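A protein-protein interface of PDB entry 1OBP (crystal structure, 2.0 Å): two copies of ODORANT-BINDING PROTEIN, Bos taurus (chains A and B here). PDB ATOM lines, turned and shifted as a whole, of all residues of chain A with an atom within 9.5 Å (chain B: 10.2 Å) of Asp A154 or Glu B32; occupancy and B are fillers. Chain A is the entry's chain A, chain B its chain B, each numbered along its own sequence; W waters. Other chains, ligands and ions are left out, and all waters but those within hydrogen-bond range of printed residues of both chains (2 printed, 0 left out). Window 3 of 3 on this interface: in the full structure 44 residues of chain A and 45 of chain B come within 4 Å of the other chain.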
ATOM      1  N   ASN A  66      28.151   2.722  14.160  1.00  0.00           N
ATOM      2  CA  ASN A  66      29.346   2.790  13.320  1.00  0.00           C
ATOM      3  C   ASN A  66      30.422   2.057  14.091  1.00  0.00           C
ATOM      4  O   ASN A  66      30.693   2.414  15.238  1.00  0.00           O
ATOM      5  CB  ASN A  66      29.746   4.233  13.074  1.00  0.00           C
ATOM      6  CG  ASN A  66      28.745   4.946  12.231  1.00  0.00           C
ATOM      7  OD1 ASN A  66      28.330   4.443  11.181  1.00  0.00           O
ATOM      8  ND2 ASN A  66      28.280   6.085  12.713  1.00  0.00           N
ATOM      9  N   VAL A 147      30.228  19.423  -1.620  1.00  0.00           N
ATOM     10  CA  VAL A 147      29.933  18.443  -0.584  1.00  0.00           C
ATOM     11  C   VAL A 147      30.487  17.066  -0.969  1.00  0.00           C
ATOM     12  O   VAL A 147      30.360  16.625  -2.117  1.00  0.00           O
ATOM     13  CB  VAL A 147      28.408  18.334  -0.349  1.00  0.00           C
ATOM     14  CG1 VAL A 147      28.102  17.269   0.690  1.00  0.00           C
ATOM     15  CG2 VAL A 147      27.834  19.672   0.070  1.00  0.00           C
ATOM     16  N   ASN A 148      31.148  16.425  -0.007  1.00  0.00           N
ATOM     17  CA  ASN A 148      31.730  15.086  -0.183  1.00  0.00           C
ATOM     18  C   ASN A 148      30.653  14.087   0.235  1.00  0.00           C
ATOM     19  O   ASN A 148      30.212  14.081   1.385  1.00  0.00           O
ATOM     20  CB  ASN A 148      32.953  14.910   0.734  1.00  0.00           C
ATOM     21  CG  ASN A 148      33.701  13.603   0.482  1.00  0.00           C
ATOM     22  OD1 ASN A 148      33.099  12.552   0.255  1.00  0.00           O
ATOM     23  ND2 ASN A 148      35.025  13.668   0.528  1.00  0.00           N
ATOM     24  N   PHE A 149      30.241  13.231  -0.679  1.00  0.00           N
ATOM     25  CA  PHE A 149      29.208  12.263  -0.344  1.00  0.00           C
ATOM     26  C   PHE A 149      29.758  10.903   0.062  1.00  0.00           C
ATOM     27  O   PHE A 149      29.014  10.046   0.555  1.00  0.00           O
ATOM     28  CB  PHE A 149      28.222  12.112  -1.517  1.00  0.00           C
ATOM     29  CG  PHE A 149      27.287  13.286  -1.682  1.00  0.00           C
ATOM     30  CD1 PHE A 149      27.731  14.475  -2.284  1.00  0.00           C
ATOM     31  CD2 PHE A 149      25.960  13.202  -1.251  1.00  0.00           C
ATOM     32  CE1 PHE A 149      26.862  15.561  -2.454  1.00  0.00           C
ATOM     33  CE2 PHE A 149      25.081  14.281  -1.418  1.00  0.00           C
ATOM     34  CZ  PHE A 149      25.539  15.467  -2.025  1.00  0.00           C
ATOM     35  N   LEU A 150      31.054  10.693  -0.128  1.00  0.00           N
ATOM     36  CA  LEU A 150      31.647   9.411   0.207  1.00  0.00           C
ATOM     37  C   LEU A 150      31.933   9.276   1.706  1.00  0.00           C
ATOM     38  O   LEU A 150      31.718   8.216   2.296  1.00  0.00           O
ATOM     39  CB  LEU A 150      32.888   9.182  -0.654  1.00  0.00           C
ATOM     40  CG  LEU A 150      32.890   8.003  -1.644  1.00  0.00           C
ATOM     41  CD1 LEU A 150      31.536   7.768  -2.294  1.00  0.00           C
ATOM     42  CD2 LEU A 150      33.955   8.204  -2.693  1.00  0.00           C
ATOM     43  N   GLU A 151      32.382  10.351   2.339  1.00  0.00           N
ATOM     44  CA  GLU A 151      32.648  10.319   3.776  1.00  0.00           C
ATOM     45  C   GLU A 151      31.796  11.393   4.439  1.00  0.00           C
ATOM     46  O   GLU A 151      32.289  12.480   4.771  1.00  0.00           O
ATOM     47  CB  GLU A 151      34.139  10.541   4.090  1.00  0.00           C
ATOM     48  CG  GLU A 151      34.746  11.806   3.483  1.00  0.00           C
ATOM     49  CD  GLU A 151      35.964  12.312   4.243  1.00  0.00           C
ATOM     50  OE1 GLU A 151      35.762  12.842   5.357  1.00  0.00           O
ATOM     51  OE2 GLU A 151      37.107  12.200   3.726  1.00  0.00           O
ATOM     52  N   ASN A 152      30.513  11.084   4.607  1.00  0.00           N
ATOM     53  CA  ASN A 152      29.558  12.014   5.207  1.00  0.00           C
ATOM     54  C   ASN A 152      28.586  11.261   6.102  1.00  0.00           C
ATOM     55  O   ASN A 152      27.923  10.319   5.669  1.00  0.00           O
ATOM     56  CB  ASN A 152      28.792  12.765   4.111  1.00  0.00           C
ATOM     57  CG  ASN A 152      28.157  14.034   4.619  1.00  0.00           C
ATOM     58  OD1 ASN A 152      28.843  15.011   4.914  1.00  0.00           O
ATOM     59  ND2 ASN A 152      26.844  14.024   4.742  1.00  0.00           N
ATOM     60  N   GLU A 153      28.504  11.691   7.354  1.00  0.00           N
ATOM     61  CA  GLU A 153      27.631  11.054   8.337  1.00  0.00           C
ATOM     62  C   GLU A 153      26.124  11.155   8.085  1.00  0.00           C
ATOM     63  O   GLU A 153      25.357  10.301   8.532  1.00  0.00           O
ATOM     64  CB  GLU A 153      27.991  11.528   9.754  1.00  0.00           C
ATOM     65  CG  GLU A 153      28.334  13.012   9.887  1.00  0.00           C
ATOM     66  CD  GLU A 153      29.187  13.322  11.121  1.00  0.00           C
ATOM     67  OE1 GLU A 153      29.704  12.372  11.756  1.00  0.00           O
ATOM     68  OE2 GLU A 153      29.350  14.524  11.452  1.00  0.00           O
ATOM     69  N   ASP A 154      25.701  12.173   7.352  1.00  0.00           N
ATOM     70  CA  ASP A 154      24.285  12.354   7.060  1.00  0.00           C
ATOM     71  C   ASP A 154      23.923  11.614   5.771  1.00  0.00           C
ATOM     72  O   ASP A 154      23.811  12.220   4.705  1.00  0.00           O
ATOM     73  CB  ASP A 154      23.978  13.854   6.944  1.00  0.00           C
ATOM     74  CG  ASP A 154      22.491  14.161   6.917  1.00  0.00           C
ATOM     75  OD1 ASP A 154      21.679  13.289   7.508  1.00  0.00           O
ATOM     76  OD2 ASP A 154      22.084  15.201   6.402  1.00  0.00           O
ATOM     77  N   HIS A 155      23.717  10.304   5.887  1.00  0.00           N
ATOM     78  CA  HIS A 155      23.385   9.451   4.738  1.00  0.00           C
ATOM     79  C   HIS A 155      22.110   8.604   4.966  1.00  0.00           C
ATOM     80  O   HIS A 155      21.611   8.513   6.094  1.00  0.00           O
ATOM     81  CB  HIS A 155      24.575   8.526   4.432  1.00  0.00           C
ATOM     82  CG  HIS A 155      24.992   7.675   5.596  1.00  0.00           C
ATOM     83  ND1 HIS A 155      24.301   6.545   5.987  1.00  0.00           N
ATOM     84  CD2 HIS A 155      26.015   7.809   6.475  1.00  0.00           C
ATOM     85  CE1 HIS A 155      24.875   6.025   7.056  1.00  0.00           C
ATOM     86  NE2 HIS A 155      25.919   6.774   7.372  1.00  0.00           N
ATOM     87  N   PRO A 156      21.558   7.997   3.894  1.00  0.00           N
ATOM     88  CA  PRO A 156      20.351   7.162   3.983  1.00  0.00           C
ATOM     89  C   PRO A 156      20.630   5.795   4.618  1.00  0.00           C
ATOM     90  O   PRO A 156      21.775   5.338   4.693  1.00  0.00           O
ATOM     91  CB  PRO A 156      19.937   6.980   2.520  1.00  0.00           C
ATOM     92  CG  PRO A 156      20.606   8.104   1.795  1.00  0.00           C
ATOM     93  CD  PRO A 156      21.938   8.201   2.484  1.00  0.00           C
ATOM     94  N   HIS A 157      19.567   5.133   5.051  1.00  0.00           N
ATOM     95  CA  HIS A 157      19.663   3.818   5.673  1.00  0.00           C
ATOM     96  C   HIS A 157      19.181   2.742   4.731  1.00  0.00           C
ATOM     97  O   HIS A 157      18.081   2.841   4.163  1.00  0.00           O
ATOM     98  CB  HIS A 157      18.810   3.749   6.930  1.00  0.00           C
ATOM     99  CG  HIS A 157      19.143   4.805   7.922  1.00  0.00           C
ATOM    100  ND1 HIS A 157      20.356   4.848   8.575  1.00  0.00           N
ATOM    101  CD2 HIS A 157      18.441   5.879   8.347  1.00  0.00           C
ATOM    102  CE1 HIS A 157      20.388   5.905   9.362  1.00  0.00           C
ATOM    103  NE2 HIS A 157      19.239   6.547   9.244  1.00  0.00           N
ATOM    104  N   THR B  19      27.215   8.949  -5.622  1.00  0.00           N
ATOM    105  CA  THR B  19      27.676  10.340  -5.703  1.00  0.00           C
ATOM    106  C   THR B  19      28.987  10.464  -4.941  1.00  0.00           C
ATOM    107  O   THR B  19      29.103   9.932  -3.829  1.00  0.00           O
ATOM    108  CB  THR B  19      26.688  11.291  -4.993  1.00  0.00           C
ATOM    109  OG1 THR B  19      25.351  11.017  -5.433  1.00  0.00           O
ATOM    110  CG2 THR B  19      27.021  12.753  -5.292  1.00  0.00           C
ATOM    111  N   ASN B  26      25.003  28.068  -5.694  1.00  0.00           N
ATOM    112  CA  ASN B  26      24.115  28.504  -4.608  1.00  0.00           C
ATOM    113  C   ASN B  26      24.215  27.420  -3.529  1.00  0.00           C
ATOM    114  O   ASN B  26      23.652  26.317  -3.657  1.00  0.00           O
ATOM    115  CB  ASN B  26      22.665  28.664  -5.116  1.00  0.00           C
ATOM    116  CG  ASN B  26      21.727  29.242  -4.072  1.00  0.00           C
ATOM    117  OD1 ASN B  26      22.061  29.332  -2.887  1.00  0.00           O
ATOM    118  ND2 ASN B  26      20.524  29.609  -4.502  1.00  0.00           N
ATOM    119  N   PRO B  27      24.979  27.702  -2.469  1.00  0.00           N
ATOM    120  CA  PRO B  27      25.166  26.752  -1.371  1.00  0.00           C
ATOM    121  C   PRO B  27      23.878  26.250  -0.729  1.00  0.00           C
ATOM    122  O   PRO B  27      23.804  25.093  -0.328  1.00  0.00           O
ATOM    123  CB  PRO B  27      26.043  27.529  -0.379  1.00  0.00           C
ATOM    124  CG  PRO B  27      25.805  28.997  -0.732  1.00  0.00           C
ATOM    125  CD  PRO B  27      25.726  28.953  -2.234  1.00  0.00           C
ATOM    126  N   GLU B  28      22.840  27.076  -0.694  1.00  0.00           N
ATOM    127  CA  GLU B  28      21.580  26.658  -0.083  1.00  0.00           C
ATOM    128  C   GLU B  28      20.985  25.401  -0.738  1.00  0.00           C
ATOM    129  O   GLU B  28      20.316  24.600  -0.085  1.00  0.00           O
ATOM    130  CB  GLU B  28      20.555  27.797  -0.130  1.00  0.00           C
ATOM    131  CG  GLU B  28      19.920  27.976  -1.491  1.00  0.00           C
ATOM    132  CD  GLU B  28      19.188  29.299  -1.659  1.00  0.00           C
ATOM    133  OE1 GLU B  28      19.557  30.288  -0.978  1.00  0.00           O
ATOM    134  OE2 GLU B  28      18.252  29.347  -2.496  1.00  0.00           O
ATOM    135  N   LYS B  29      21.254  25.216  -2.020  1.00  0.00           N
ATOM    136  CA  LYS B  29      20.706  24.074  -2.730  1.00  0.00           C
ATOM    137  C   LYS B  29      21.265  22.714  -2.307  1.00  0.00           C
ATOM    138  O   LYS B  29      20.609  21.688  -2.517  1.00  0.00           O
ATOM    139  CB  LYS B  29      20.886  24.265  -4.245  1.00  0.00           C
ATOM    140  CG  LYS B  29      20.208  25.506  -4.798  1.00  0.00           C
ATOM    141  CD  LYS B  29      18.709  25.443  -4.595  1.00  0.00           C
ATOM    142  CE  LYS B  29      18.023  26.650  -5.203  1.00  0.00           C
ATOM    143  NZ  LYS B  29      16.546  26.544  -5.069  1.00  0.00           N
ATOM    144  N   ILE B  30      22.485  22.703  -1.765  1.00  0.00           N
ATOM    145  CA  ILE B  30      23.130  21.452  -1.358  1.00  0.00           C
ATOM    146  C   ILE B  30      23.372  21.306   0.132  1.00  0.00           C
ATOM    147  O   ILE B  30      24.072  20.396   0.566  1.00  0.00           O
ATOM    148  CB  ILE B  30      24.453  21.173  -2.130  1.00  0.00           C
ATOM    149  CG1 ILE B  30      25.432  22.329  -1.988  1.00  0.00           C
ATOM    150  CG2 ILE B  30      24.175  20.909  -3.595  1.00  0.00           C
ATOM    151  CD1 ILE B  30      26.724  22.096  -2.754  1.00  0.00           C
ATOM    152  N   GLN B  31      22.784  22.210   0.904  1.00  0.00           N
ATOM    153  CA  GLN B  31      22.875  22.175   2.345  1.00  0.00           C
ATOM    154  C   GLN B  31      21.907  21.128   2.831  1.00  0.00           C
ATOM    155  O   GLN B  31      21.076  20.641   2.065  1.00  0.00           O
ATOM    156  CB  GLN B  31      22.436  23.505   2.939  1.00  0.00           C
ATOM    157  CG  GLN B  31      23.376  24.631   2.651  1.00  0.00           C
ATOM    158  CD  GLN B  31      24.778  24.382   3.172  1.00  0.00           C
ATOM    159  OE1 GLN B  31      25.094  23.311   3.717  1.00  0.00           O
ATOM    160  NE2 GLN B  31      25.631  25.385   3.028  1.00  0.00           N
ATOM    161  N   GLU B  32      21.971  20.829   4.125  1.00  0.00           N
ATOM    162  CA  GLU B  32      21.080  19.848   4.728  1.00  0.00           C
ATOM    163  C   GLU B  32      19.655  20.295   4.432  1.00  0.00           C
ATOM    164  O   GLU B  32      19.295  21.435   4.710  1.00  0.00           O
ATOM    165  CB  GLU B  32      21.324  19.778   6.233  1.00  0.00           C
ATOM    166  CG  GLU B  32      20.645  18.596   6.895  1.00  0.00           C
ATOM    167  CD  GLU B  32      21.370  18.149   8.138  1.00  0.00           C
ATOM    168  OE1 GLU B  32      22.431  17.494   8.006  1.00  0.00           O
ATOM    169  OE2 GLU B  32      20.882  18.470   9.244  1.00  0.00           O
ATOM    170  N   ASN B  33      18.871  19.398   3.841  1.00  0.00           N
ATOM    171  CA  ASN B  33      17.487  19.657   3.436  1.00  0.00           C
ATOM    172  C   ASN B  33      17.399  20.455   2.138  1.00  0.00           C
ATOM    173  O   ASN B  33      16.332  20.958   1.773  1.00  0.00           O
ATOM    174  CB  ASN B  33      16.667  20.303   4.550  1.00  0.00           C
ATOM    175  CG  ASN B  33      16.284  19.310   5.632  1.00  0.00           C
ATOM    176  OD1 ASN B  33      15.367  18.500   5.456  1.00  0.00           O
ATOM    177  ND2 ASN B  33      16.998  19.350   6.754  1.00  0.00           N
ATOM    178  N   GLY B  34      18.520  20.532   1.421  1.00  0.00           N
ATOM    179  CA  GLY B  34      18.565  21.228   0.151  1.00  0.00           C
ATOM    180  C   GLY B  34      18.140  20.183  -0.863  1.00  0.00           C
ATOM    181  O   GLY B  34      18.506  19.013  -0.708  1.00  0.00           O
ATOM    182  N   PRO B  35      17.412  20.561  -1.930  1.00  0.00           N
ATOM    183  CA  PRO B  35      16.968  19.580  -2.920  1.00  0.00           C
ATOM    184  C   PRO B  35      18.021  18.923  -3.804  1.00  0.00           C
ATOM    185  O   PRO B  35      17.728  17.915  -4.466  1.00  0.00           O
ATOM    186  CB  PRO B  35      15.917  20.352  -3.719  1.00  0.00           C
ATOM    187  CG  PRO B  35      16.387  21.746  -3.638  1.00  0.00           C
ATOM    188  CD  PRO B  35      16.826  21.885  -2.210  1.00  0.00           C
ATOM    189  N   PHE B  36      19.244  19.455  -3.815  1.00  0.00           N
ATOM    190  CA  PHE B  36      20.278  18.855  -4.651  1.00  0.00           C
ATOM    191  C   PHE B  36      21.355  18.104  -3.869  1.00  0.00           C
ATOM    192  O   PHE B  36      22.439  17.857  -4.391  1.00  0.00           O
ATOM    193  CB  PHE B  36      20.886  19.869  -5.642  1.00  0.00           C
ATOM    194  CG  PHE B  36      19.993  20.160  -6.841  1.00  0.00           C
ATOM    195  CD1 PHE B  36      20.072  19.375  -7.992  1.00  0.00           C
ATOM    196  CD2 PHE B  36      19.041  21.197  -6.793  1.00  0.00           C
ATOM    197  CE1 PHE B  36      19.214  19.610  -9.084  1.00  0.00           C
ATOM    198  CE2 PHE B  36      18.178  21.444  -7.872  1.00  0.00           C
ATOM    199  CZ  PHE B  36      18.267  20.650  -9.020  1.00  0.00           C
ATOM    200  N   ARG B  37      21.089  17.798  -2.602  1.00  0.00           N
ATOM    201  CA  ARG B  37      22.045  17.013  -1.823  1.00  0.00           C
ATOM    202  C   ARG B  37      21.571  15.563  -2.028  1.00  0.00           C
ATOM    203  O   ARG B  37      21.054  14.904  -1.119  1.00  0.00           O
ATOM    204  CB  ARG B  37      22.030  17.423  -0.351  1.00  0.00           C
ATOM    205  CG  ARG B  37      23.008  16.597   0.499  1.00  0.00           C
ATOM    206  CD  ARG B  37      22.827  16.860   1.980  1.00  0.00           C
ATOM    207  NE  ARG B  37      23.505  18.078   2.368  1.00  0.00           N
ATOM    208  CZ  ARG B  37      24.577  18.134   3.155  1.00  0.00           C
ATOM    209  NH1 ARG B  37      25.110  17.028   3.668  1.00  0.00           N
ATOM    210  NH2 ARG B  37      25.154  19.306   3.372  1.00  0.00           N
ATOM    211  N   THR B  38      21.730  15.106  -3.259  1.00  0.00           N
ATOM    212  CA  THR B  38      21.271  13.797  -3.713  1.00  0.00           C
ATOM    213  C   THR B  38      22.260  12.633  -3.669  1.00  0.00           C
ATOM    214  O   THR B  38      23.317  12.665  -4.306  1.00  0.00           O
ATOM    215  CB  THR B  38      20.745  13.919  -5.173  1.00  0.00           C
ATOM    216  OG1 THR B  38      21.834  14.275  -6.049  1.00  0.00           O
ATOM    217  CG2 THR B  38      19.687  15.012  -5.252  1.00  0.00           C
ATOM    218  N   TYR B  39      21.863  11.563  -2.994  1.00  0.00           N
ATOM    219  CA  TYR B  39      22.682  10.362  -2.932  1.00  0.00           C
ATOM    220  C   TYR B  39      22.169   9.438  -4.038  1.00  0.00           C
ATOM    221  O   TYR B  39      21.038   8.980  -3.951  1.00  0.00           O
ATOM    222  CB  TYR B  39      22.498   9.701  -1.571  1.00  0.00           C
ATOM    223  CG  TYR B  39      23.310  10.336  -0.473  1.00  0.00           C
ATOM    224  CD1 TYR B  39      22.809  11.416   0.266  1.00  0.00           C
ATOM    225  CD2 TYR B  39      24.573   9.844  -0.152  1.00  0.00           C
ATOM    226  CE1 TYR B  39      23.560  11.994   1.313  1.00  0.00           C
ATOM    227  CE2 TYR B  39      25.324  10.401   0.884  1.00  0.00           C
ATOM    228  CZ  TYR B  39      24.815  11.470   1.612  1.00  0.00           C
ATOM    229  OH  TYR B  39      25.571  11.999   2.630  1.00  0.00           O
ATOM    230  N   SER B  57      18.121   9.502  -3.433  1.00  0.00           N
ATOM    231  CA  SER B  57      17.490   9.795  -2.154  1.00  0.00           C
ATOM    232  C   SER B  57      17.953  11.161  -1.695  1.00  0.00           C
ATOM    233  O   SER B  57      19.115  11.539  -1.912  1.00  0.00           O
ATOM    234  CB  SER B  57      17.895   8.764  -1.079  1.00  0.00           C
ATOM    235  OG  SER B  57      17.564   7.434  -1.465  1.00  0.00           O
ATOM    236  N   VAL B  58      17.070  11.873  -0.997  1.00  0.00           N
ATOM    237  CA  VAL B  58      17.380  13.211  -0.515  1.00  0.00           C
ATOM    238  C   VAL B  58      16.547  13.456   0.730  1.00  0.00           C
ATOM    239  O   VAL B  58      15.484  12.867   0.900  1.00  0.00           O
ATOM    240  CB  VAL B  58      17.158  14.297  -1.677  1.00  0.00           C
ATOM    241  CG1 VAL B  58      15.795  14.146  -2.336  1.00  0.00           C
ATOM    242  CG2 VAL B  58      17.353  15.698  -1.164  1.00  0.00           C
ATOM    243  N   LYS B  59      17.073  14.231   1.658  1.00  0.00           N
ATOM    244  CA  LYS B  59      16.354  14.509   2.891  1.00  0.00           C
ATOM    245  C   LYS B  59      15.548  15.803   2.755  1.00  0.00           C
ATOM    246  O   LYS B  59      16.030  16.788   2.189  1.00  0.00           O
ATOM    247  CB  LYS B  59      17.331  14.586   4.069  1.00  0.00           C
ATOM    248  CG  LYS B  59      16.697  14.260   5.403  1.00  0.00           C
ATOM    249  CD  LYS B  59      17.734  13.821   6.416  1.00  0.00           C
ATOM    250  CE  LYS B  59      18.404  14.991   7.070  1.00  0.00           C
ATOM    251  NZ  LYS B  59      17.393  15.792   7.813  1.00  0.00           N
ATOM    252  N   ARG B  60      14.311  15.765   3.244  1.00  0.00           N
ATOM    253  CA  ARG B  60      13.385  16.890   3.197  1.00  0.00           C
ATOM    254  C   ARG B  60      12.550  16.832   4.472  1.00  0.00           C
ATOM    255  O   ARG B  60      11.981  15.789   4.801  1.00  0.00           O
ATOM    256  CB  ARG B  60      12.490  16.754   1.965  1.00  0.00           C
ATOM    257  CG  ARG B  60      11.489  17.877   1.738  1.00  0.00           C
ATOM    258  CD  ARG B  60      10.132  17.592   2.380  1.00  0.00           C
ATOM    259  NE  ARG B  60       9.603  16.261   2.055  1.00  0.00           N
ATOM    260  CZ  ARG B  60       9.219  15.857   0.842  1.00  0.00           C
ATOM    261  NH1 ARG B  60       9.292  16.671  -0.207  1.00  0.00           N
ATOM    262  NH2 ARG B  60       8.755  14.624   0.678  1.00  0.00           N
ATOM    263  N   ASP B  61      12.491  17.940   5.202  1.00  0.00           N
ATOM    264  CA  ASP B  61      11.735  17.985   6.456  1.00  0.00           C
ATOM    265  C   ASP B  61      12.319  16.926   7.384  1.00  0.00           C
ATOM    266  O   ASP B  61      11.586  16.185   8.038  1.00  0.00           O
ATOM    267  CB  ASP B  61      10.241  17.701   6.220  1.00  0.00           C
ATOM    268  CG  ASP B  61       9.387  17.906   7.484  1.00  0.00           C
ATOM    269  OD1 ASP B  61       9.107  19.079   7.841  1.00  0.00           O
ATOM    270  OD2 ASP B  61       8.991  16.897   8.122  1.00  0.00           O
ATOM    271  N   GLY B  62      13.643  16.816   7.383  1.00  0.00           N
ATOM    272  CA  GLY B  62      14.307  15.841   8.232  1.00  0.00           C
ATOM    273  C   GLY B  62      14.010  14.375   7.925  1.00  0.00           C
ATOM    274  O   GLY B  62      14.304  13.503   8.744  1.00  0.00           O
ATOM    275  N   LYS B  63      13.483  14.082   6.739  1.00  0.00           N
ATOM    276  CA  LYS B  63      13.169  12.711   6.383  1.00  0.00           C
ATOM    277  C   LYS B  63      13.713  12.329   5.016  1.00  0.00           C
ATOM    278  O   LYS B  63      13.643  13.106   4.077  1.00  0.00           O
ATOM    279  CB  LYS B  63      11.660  12.510   6.428  1.00  0.00           C
ATOM    280  CG  LYS B  63      11.098  12.481   7.825  1.00  0.00           C
ATOM    281  CD  LYS B  63       9.582  12.519   7.808  1.00  0.00           C
ATOM    282  CE  LYS B  63       9.090  13.896   7.387  1.00  0.00           C
ATOM    283  NZ  LYS B  63       7.695  14.187   7.850  1.00  0.00           N
ATOM    284  N   TRP B  64      14.252  11.124   4.899  1.00  0.00           N
ATOM    285  CA  TRP B  64      14.791  10.663   3.626  1.00  0.00           C
ATOM    286  C   TRP B  64      13.678  10.238   2.684  1.00  0.00           C
ATOM    287  O   TRP B  64      12.775   9.496   3.084  1.00  0.00           O
ATOM    288  CB  TRP B  64      15.779   9.514   3.836  1.00  0.00           C
ATOM    289  CG  TRP B  64      17.094   9.951   4.410  1.00  0.00           C
ATOM    290  CD1 TRP B  64      17.493   9.866   5.713  1.00  0.00           C
ATOM    291  CD2 TRP B  64      18.185  10.536   3.693  1.00  0.00           C
ATOM    292  NE1 TRP B  64      18.770  10.361   5.851  1.00  0.00           N
ATOM    293  CE2 TRP B  64      19.218  10.780   4.628  1.00  0.00           C
ATOM    294  CE3 TRP B  64      18.390  10.876   2.344  1.00  0.00           C
ATOM    295  CZ2 TRP B  64      20.445  11.351   4.258  1.00  0.00           C
ATOM    296  CZ3 TRP B  64      19.609  11.445   1.972  1.00  0.00           C
ATOM    297  CH2 TRP B  64      20.619  11.677   2.929  1.00  0.00           C
HETATM  298  O   HOH W   1      27.756   8.171  -1.939  1.00  0.00           O
HETATM  299  O   HOH W   2      18.920  12.287   8.650  1.00  0.00           O
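Printed residues of chain B within 4 Å of Phe A149: Thr B19 (3.3 Å), Arg B37 (3.7 Å), Thr B38 (3.8 Å) and Tyr B39 (3.5 Å).
Asn A152 touches just these residues of chain B: Arg B37 (3.6 Å) and Tyr B39 (3.2 Å).
Of chain B, only Tyr B39 (3.96 Å) and Trp B64 (3.3 Å) come within 4 Å of His A155.
Asn B26 touches none of the printed residues of chain A.
No residue of chain A comes within 4 Å of Asn B33.
Printed residues of chain A within 4 Å of Arg B37: Phe A149 (3.7 Å) and Asn A152 (3.6 Å).
The nearest printed residue of chain B that does not touch Leu A150 is Tyr B39 (5.8 Å).
No position is printed for both chains.
Of the 16 pairs that touch across the chains among the printed residues, none has its exchanged pair printed and touching as well.
Of the 23 printed residues of chain B, 8 touch a printed residue of chain A.
Hydrophobic or aromatic side chains of chain B that line the printed part of chain A: Ile B30, Tyr B39 and Trp B64.
Of the 12 printed residues of chain A, 7 touch a printed residue of chain B.
Hydrophobic or aromatic side chains of chain A that line the printed part of chain B: Val A147, Phe A149, Leu A150 and Pro A156.
Among the printed residues, 16 pairs touch across the chains.
Among the printed residues, no Asp or Glu carboxylate lies within 4 Å of a Lys or Arg side-chain nitrogen of the other chain.
ND2 of Asn A152 is in hydrogen-bond range of OH of Tyr B39 (3.2 Å).
The side-chain hydroxyl (OH) of Tyr B39 sits at hydrogen-bond distance from the backbone carbonyl oxygen (O) of Asp A154.
O of His A155 sits at hydrogen-bond distance from NE1 of Trp B64, at 3.4 Å.
OD2 of Asp A154 sits close to OE1 of Glu B32, 2.8 Å away.
CG2 of Val A147 touches O of Ile B30 (3.9 Å).
O of Thr B19 touches CB of Phe A149, at 3.3 Å.
CG of Arg B37 touches CE2 of Phe A149 (3.7 Å).
Phe A149 touches Thr B38 (CE2 to O, 3.8 Å).
Leu A150 touches Thr B19 (CD1 to O, 3.6 Å).
ND2 of Asn A152 touches NH1 of Arg B37, 3.6 Å away.
Trp B64 touches Asp A154.
His A155 touches Tyr B39.
Pro A156 touches Tyr B39.
Trp B64 touches Pro A156.
Water W1 lies within hydrogen-bond range of O of Thr B19 (2.9 Å) and O of Phe A149 (3.4 Å).
Water W2 bridges the side-chain carboxylate of Asp A154 and the indole nitrogen of Trp B64.
The side-chain amide oxygen of Asn A148 lies within hydrogen-bond range of the backbone NH of Leu A150, 2.8 Å away.
ND2 of Asn A152 sits close to N of Asp A154 (3.4 Å).
OG1 of Thr B19 sits at hydrogen-bond distance from O of Thr B38 (2.9 Å).
The backbone carbonyl oxygen (O) of Ile B30 is in hydrogen-bond range of the guanidinium group (NE) of Arg B37 (3.0 Å).
The backbone NH (N) of Tyr B39 is in hydrogen-bond range of the backbone carbonyl oxygen (O) of Ser B57 (3.0 Å).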
